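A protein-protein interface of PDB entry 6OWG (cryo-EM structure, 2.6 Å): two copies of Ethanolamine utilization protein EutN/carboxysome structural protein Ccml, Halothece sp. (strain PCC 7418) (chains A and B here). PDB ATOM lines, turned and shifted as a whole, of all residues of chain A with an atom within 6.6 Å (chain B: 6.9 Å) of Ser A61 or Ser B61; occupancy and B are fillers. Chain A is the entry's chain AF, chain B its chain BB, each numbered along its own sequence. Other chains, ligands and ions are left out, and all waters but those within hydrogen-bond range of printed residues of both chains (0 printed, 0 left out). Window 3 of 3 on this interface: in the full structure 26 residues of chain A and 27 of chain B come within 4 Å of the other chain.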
ATOM      1  N   ASN A  58      -9.843  10.020  29.250  1.00  0.00           N
ATOM      2  CA  ASN A  58      -9.313  10.926  30.250  1.00  0.00           C
ATOM      3  C   ASN A  58     -10.156  12.198  30.285  1.00  0.00           C
ATOM      4  O   ASN A  58     -11.070  12.389  29.481  1.00  0.00           O
ATOM      5  CB  ASN A  58      -7.824  11.200  29.999  1.00  0.00           C
ATOM      6  CG  ASN A  58      -7.534  11.777  28.622  1.00  0.00           C
ATOM      7  OD1 ASN A  58      -8.426  12.069  27.835  1.00  0.00           O
ATOM      8  ND2 ASN A  58      -6.259  11.944  28.332  1.00  0.00           N
ATOM      9  N   ARG A  59      -9.846  13.083  31.224  1.00  0.00           N
ATOM     10  CA  ARG A  59     -10.598  14.313  31.377  1.00  0.00           C
ATOM     11  C   ARG A  59      -9.617  15.461  31.536  1.00  0.00           C
ATOM     12  O   ARG A  59      -8.505  15.288  32.037  1.00  0.00           O
ATOM     13  CB  ARG A  59     -11.547  14.241  32.578  1.00  0.00           C
ATOM     14  CG  ARG A  59     -12.805  15.062  32.419  1.00  0.00           C
ATOM     15  CD  ARG A  59     -13.785  14.804  33.551  1.00  0.00           C
ATOM     16  NE  ARG A  59     -13.428  15.533  34.763  1.00  0.00           N
ATOM     17  CZ  ARG A  59     -14.059  15.399  35.924  1.00  0.00           C
ATOM     18  NH1 ARG A  59     -15.081  14.565  36.032  1.00  0.00           N
ATOM     19  NH2 ARG A  59     -13.671  16.105  36.974  1.00  0.00           N
ATOM     20  N   GLY A  60     -10.036  16.637  31.082  1.00  0.00           N
ATOM     21  CA  GLY A  60      -9.286  17.846  31.340  1.00  0.00           C
ATOM     22  C   GLY A  60      -8.194  18.139  30.338  1.00  0.00           C
ATOM     23  O   GLY A  60      -8.351  17.892  29.141  1.00  0.00           O
ATOM     24  N   SER A  61      -7.069  18.661  30.826  1.00  0.00           N
ATOM     25  CA  SER A  61      -5.964  19.070  29.970  1.00  0.00           C
ATOM     26  C   SER A  61      -5.155  17.899  29.442  1.00  0.00           C
ATOM     27  O   SER A  61      -4.283  18.103  28.593  1.00  0.00           O
ATOM     28  CB  SER A  61      -5.047  20.028  30.728  1.00  0.00           C
ATOM     29  OG  SER A  61      -4.423  19.385  31.822  1.00  0.00           O
ATOM     30  N   ALA A  62      -5.417  16.684  29.927  1.00  0.00           N
ATOM     31  CA  ALA A  62      -4.769  15.493  29.400  1.00  0.00           C
ATOM     32  C   ALA A  62      -5.270  15.138  28.010  1.00  0.00           C
ATOM     33  O   ALA A  62      -4.589  14.407  27.286  1.00  0.00           O
ATOM     34  CB  ALA A  62      -4.990  14.322  30.353  1.00  0.00           C
ATOM     35  N   ALA A  63      -6.434  15.657  27.612  1.00  0.00           N
ATOM     36  CA  ALA A  63      -6.960  15.423  26.274  1.00  0.00           C
ATOM     37  C   ALA A  63      -6.193  16.185  25.203  1.00  0.00           C
ATOM     38  O   ALA A  63      -6.369  15.900  24.015  1.00  0.00           O
ATOM     39  CB  ALA A  63      -8.434  15.808  26.225  1.00  0.00           C
ATOM     40  N   ARG A  64      -5.348  17.137  25.593  1.00  0.00           N
ATOM     41  CA  ARG A  64      -4.593  17.965  24.666  1.00  0.00           C
ATOM     42  C   ARG A  64      -3.116  17.603  24.620  1.00  0.00           C
ATOM     43  O   ARG A  64      -2.284  18.471  24.345  1.00  0.00           O
ATOM     44  CB  ARG A  64      -4.746  19.436  25.040  1.00  0.00           C
ATOM     45  CG  ARG A  64      -6.156  19.948  24.970  1.00  0.00           C
ATOM     46  CD  ARG A  64      -6.190  21.429  25.238  1.00  0.00           C
ATOM     47  NE  ARG A  64      -6.539  21.713  26.622  1.00  0.00           N
ATOM     48  CZ  ARG A  64      -5.706  22.257  27.498  1.00  0.00           C
ATOM     49  NH1 ARG A  64      -4.475  22.580  27.138  1.00  0.00           N
ATOM     50  NH2 ARG A  64      -6.109  22.480  28.731  1.00  0.00           N
ATOM     51  N   GLN A  65      -2.770  16.347  24.883  1.00  0.00           N
ATOM     52  CA  GLN A  65      -1.374  15.944  24.982  1.00  0.00           C
ATOM     53  C   GLN A  65      -0.897  15.095  23.814  1.00  0.00           C
ATOM     54  O   GLN A  65       0.290  14.767  23.750  1.00  0.00           O
ATOM     55  CB  GLN A  65      -1.140  15.170  26.282  1.00  0.00           C
ATOM     56  CG  GLN A  65      -1.562  15.904  27.540  1.00  0.00           C
ATOM     57  CD  GLN A  65      -0.866  17.232  27.711  1.00  0.00           C
ATOM     58  OE1 GLN A  65       0.357  17.313  27.661  1.00  0.00           O
ATOM     59  NE2 GLN A  65      -1.644  18.284  27.931  1.00  0.00           N
ATOM     60  N   PRO A  73      -9.923  22.809  21.664  1.00  0.00           N
ATOM     61  CA  PRO A  73     -10.742  22.929  22.887  1.00  0.00           C
ATOM     62  C   PRO A  73     -11.386  21.611  23.298  1.00  0.00           C
ATOM     63  O   PRO A  73     -12.600  21.410  23.231  1.00  0.00           O
ATOM     64  CB  PRO A  73     -11.770  23.988  22.479  1.00  0.00           C
ATOM     65  CG  PRO A  73     -11.924  23.800  21.024  1.00  0.00           C
ATOM     66  CD  PRO A  73     -10.577  23.432  20.505  1.00  0.00           C
ATOM     67  N   LEU A  74     -10.557  20.679  23.757  1.00  0.00           N
ATOM     68  CA  LEU A  74     -10.988  19.331  24.101  1.00  0.00           C
ATOM     69  C   LEU A  74     -10.715  19.069  25.573  1.00  0.00           C
ATOM     70  O   LEU A  74      -9.629  19.381  26.071  1.00  0.00           O
ATOM     71  CB  LEU A  74     -10.267  18.297  23.239  1.00  0.00           C
ATOM     72  CG  LEU A  74     -10.571  18.373  21.746  1.00  0.00           C
ATOM     73  CD1 LEU A  74      -9.611  17.509  20.974  1.00  0.00           C
ATOM     74  CD2 LEU A  74     -11.992  17.945  21.482  1.00  0.00           C
ATOM     75  N   ASP A  75     -11.698  18.497  26.264  1.00  0.00           N
ATOM     76  CA  ASP A  75     -11.549  18.130  27.666  1.00  0.00           C
ATOM     77  C   ASP A  75     -11.851  16.659  27.915  1.00  0.00           C
ATOM     78  O   ASP A  75     -12.017  16.259  29.071  1.00  0.00           O
ATOM     79  CB  ASP A  75     -12.438  19.009  28.551  1.00  0.00           C
ATOM     80  CG  ASP A  75     -13.912  18.778  28.310  1.00  0.00           C
ATOM     81  OD1 ASP A  75     -14.281  18.479  27.163  1.00  0.00           O
ATOM     82  OD2 ASP A  75     -14.706  18.897  29.265  1.00  0.00           O
ATOM     83  N   ASN B  58     -17.387  22.289  26.634  1.00  0.00           N
ATOM     84  CA  ASN B  58     -16.268  21.733  27.366  1.00  0.00           C
ATOM     85  C   ASN B  58     -16.091  22.501  28.671  1.00  0.00           C
ATOM     86  O   ASN B  58     -16.779  23.488  28.934  1.00  0.00           O
ATOM     87  CB  ASN B  58     -14.999  21.725  26.502  1.00  0.00           C
ATOM     88  CG  ASN B  58     -14.579  23.107  26.013  1.00  0.00           C
ATOM     89  OD1 ASN B  58     -15.188  24.124  26.320  1.00  0.00           O
ATOM     90  ND2 ASN B  58     -13.519  23.133  25.234  1.00  0.00           N
ATOM     91  N   ARG B  59     -15.159  22.052  29.501  1.00  0.00           N
ATOM     92  CA  ARG B  59     -14.864  22.770  30.725  1.00  0.00           C
ATOM     93  C   ARG B  59     -13.373  22.724  30.995  1.00  0.00           C
ATOM     94  O   ARG B  59     -12.631  21.957  30.380  1.00  0.00           O
ATOM     95  CB  ARG B  59     -15.640  22.212  31.918  1.00  0.00           C
ATOM     96  CG  ARG B  59     -15.410  20.753  32.195  1.00  0.00           C
ATOM     97  CD  ARG B  59     -16.122  20.362  33.464  1.00  0.00           C
ATOM     98  NE  ARG B  59     -16.156  18.920  33.661  1.00  0.00           N
ATOM     99  CZ  ARG B  59     -16.603  18.333  34.764  1.00  0.00           C
ATOM    100  NH1 ARG B  59     -17.036  19.068  35.778  1.00  0.00           N
ATOM    101  NH2 ARG B  59     -16.607  17.012  34.857  1.00  0.00           N
ATOM    102  N   GLY B  60     -12.945  23.570  31.925  1.00  0.00           N
ATOM    103  CA  GLY B  60     -11.558  23.625  32.325  1.00  0.00           C
ATOM    104  C   GLY B  60     -10.746  24.579  31.482  1.00  0.00           C
ATOM    105  O   GLY B  60     -11.258  25.594  31.009  1.00  0.00           O
ATOM    106  N   SER B  61      -9.474  24.253  31.276  1.00  0.00           N
ATOM    107  CA  SER B  61      -8.591  25.090  30.481  1.00  0.00           C
ATOM    108  C   SER B  61      -8.789  24.901  28.986  1.00  0.00           C
ATOM    109  O   SER B  61      -8.131  25.589  28.201  1.00  0.00           O
ATOM    110  CB  SER B  61      -7.138  24.809  30.855  1.00  0.00           C
ATOM    111  OG  SER B  61      -6.901  23.420  30.969  1.00  0.00           O
ATOM    112  N   ALA B  62      -9.670  23.987  28.579  1.00  0.00           N
ATOM    113  CA  ALA B  62     -10.011  23.821  27.176  1.00  0.00           C
ATOM    114  C   ALA B  62     -10.883  24.954  26.662  1.00  0.00           C
ATOM    115  O   ALA B  62     -10.954  25.166  25.449  1.00  0.00           O
ATOM    116  CB  ALA B  62     -10.712  22.483  26.969  1.00  0.00           C
ATOM    117  N   ALA B  63     -11.536  25.696  27.560  1.00  0.00           N
ATOM    118  CA  ALA B  63     -12.288  26.882  27.176  1.00  0.00           C
ATOM    119  C   ALA B  63     -11.388  28.019  26.718  1.00  0.00           C
ATOM    120  O   ALA B  63     -11.874  28.957  26.080  1.00  0.00           O
ATOM    121  CB  ALA B  63     -13.151  27.347  28.345  1.00  0.00           C
ATOM    122  N   ARG B  64     -10.094  27.957  27.026  1.00  0.00           N
ATOM    123  CA  ARG B  64      -9.140  29.004  26.702  1.00  0.00           C
ATOM    124  C   ARG B  64      -8.236  28.637  25.534  1.00  0.00           C
ATOM    125  O   ARG B  64      -7.101  29.115  25.467  1.00  0.00           O
ATOM    126  CB  ARG B  64      -8.296  29.329  27.930  1.00  0.00           C
ATOM    127  CG  ARG B  64      -9.104  29.688  29.153  1.00  0.00           C
ATOM    128  CD  ARG B  64      -8.212  30.231  30.241  1.00  0.00           C
ATOM    129  NE  ARG B  64      -7.803  29.213  31.200  1.00  0.00           N
ATOM    130  CZ  ARG B  64      -6.590  28.676  31.233  1.00  0.00           C
ATOM    131  NH1 ARG B  64      -5.674  29.054  30.356  1.00  0.00           N
ATOM    132  NH2 ARG B  64      -6.291  27.767  32.140  1.00  0.00           N
ATOM    133  N   GLN B  65      -8.712  27.802  24.613  1.00  0.00           N
ATOM    134  CA  GLN B  65      -7.885  27.309  23.521  1.00  0.00           C
ATOM    135  C   GLN B  65      -8.210  27.931  22.172  1.00  0.00           C
ATOM    136  O   GLN B  65      -7.506  27.658  21.197  1.00  0.00           O
ATOM    137  CB  GLN B  65      -8.015  25.787  23.402  1.00  0.00           C
ATOM    138  CG  GLN B  65      -7.587  25.012  24.629  1.00  0.00           C
ATOM    139  CD  GLN B  65      -6.209  25.388  25.114  1.00  0.00           C
ATOM    140  OE1 GLN B  65      -5.235  25.289  24.377  1.00  0.00           O
ATOM    141  NE2 GLN B  65      -6.118  25.812  26.368  1.00  0.00           N
ATOM    142  N   LEU B  74     -12.227  31.991  31.784  1.00  0.00           N
ATOM    143  CA  LEU B  74     -13.344  31.174  31.333  1.00  0.00           C
ATOM    144  C   LEU B  74     -13.039  29.712  31.610  1.00  0.00           C
ATOM    145  O   LEU B  74     -11.936  29.239  31.323  1.00  0.00           O
ATOM    146  CB  LEU B  74     -13.605  31.384  29.841  1.00  0.00           C
ATOM    147  CG  LEU B  74     -14.069  32.779  29.430  1.00  0.00           C
ATOM    148  CD1 LEU B  74     -13.932  32.951  27.940  1.00  0.00           C
ATOM    149  CD2 LEU B  74     -15.499  33.005  29.858  1.00  0.00           C
ATOM    150  N   ASP B  75     -14.018  29.001  32.167  1.00  0.00           N
ATOM    151  CA  ASP B  75     -13.889  27.574  32.425  1.00  0.00           C
ATOM    152  C   ASP B  75     -15.012  26.770  31.788  1.00  0.00           C
ATOM    153  O   ASP B  75     -15.256  25.635  32.202  1.00  0.00           O
ATOM    154  CB  ASP B  75     -13.835  27.300  33.931  1.00  0.00           C
ATOM    155  CG  ASP B  75     -15.130  27.642  34.635  1.00  0.00           C
ATOM    156  OD1 ASP B  75     -15.809  28.580  34.190  1.00  0.00           O
ATOM    157  OD2 ASP B  75     -15.470  26.972  35.631  1.00  0.00           O
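Of chain B, only Ser B61 (3.9 Å) comes within 4 Å of Ser A61.
Of chain A, only Ser A61 and Arg A64 come within 4 Å of Ser B61.
Printed residues of chain A within 4 Å of Ala B62: Arg A64, Pro A73 and Leu A74.
Printed residues of chain B within 4 Å of Pro A73: Asn B58, Ala B62 and Gln B65.
Printed residues of chain A within 4 Å of Gln B65: Arg A64 and Pro A73.
The nearest residue of chain B that does not touch Ser A61 is Ala B62 (6.3 Å).
The guanidinium group (NH1) of Arg A59 sits close to the guanidinium group (NH2) of Arg B59, at 3.1 Å.
The side-chain amide nitrogen (ND2) of Asn B58 lies within hydrogen-bond range of the backbone carbonyl oxygen (O) of Pro A73, at 2.8 Å.
NH2 of Arg A64 is in hydrogen-bond range of OG of Ser B61.
The side-chain carboxylate (OD2) of Asp A75 is in hydrogen-bond range of the backbone NH (N) of Arg B59 (3.2 Å).
Ser A61 touches Ser B61 (CB to OG, 3.9 Å).
Arg A64 touches Ala B62 (NH2 to N, 3.9 Å).
NH1 of Arg A64 touches NE2 of Gln B65, at 3.7 Å.
Pro A73 touches Ala B62.
Pro A73 touches Gln B65 (N to CB, 3.9 Å).
Ala B62 touches Leu A74 (CB to O, 3.4 Å).
Asn B58 touches Asp A75 (CB to OD1, 3.4 Å).
The backbone NH of Gly A60 is in hydrogen-bond range of the backbone carbonyl oxygen of Asp A75.
The side-chain amide nitrogen of Gln B65 lies within hydrogen-bond range of the backbone carbonyl oxygen of Ser B61 (2.7 Å).
The backbone carbonyl oxygen (O) of Ser A61 sits at hydrogen-bond distance from the side-chain amide nitrogen (NE2) of Gln A65, at 2.7 Å.
The side-chain amide nitrogen (ND2) of Asn B58 sits at hydrogen-bond distance from the backbone carbonyl oxygen (O) of Ala B62 (3.3 Å).
Arg A59 touches its own counterpart, Arg B59.
Arg A64 touches Ser B61, but with the chains exchanged Ser A61 does not touch Arg B64 (8.0 Å).
Asp A75 touches Asn B58, but with the chains exchanged Asn A58 does not touch Asp B75 (14.2 Å).
Asp A75 touches Arg B59, but with the chains exchanged Arg A59 does not touch Asp B75 (10.6 Å).
Of the 11 pairs that touch across the chains among the printed residues, 2 have their exchanged pair printed and touching as well.
Of the 10 printed residues of chain B, 5 touch a printed residue of chain A.
Hydrophobic or aromatic side chains of chain A within 4 Å of the printed part of chain B: Pro A73.
Among the printed residues, no Asp or Glu carboxylate lies within 4 Å of a Lys or Arg side-chain nitrogen of the other chain.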
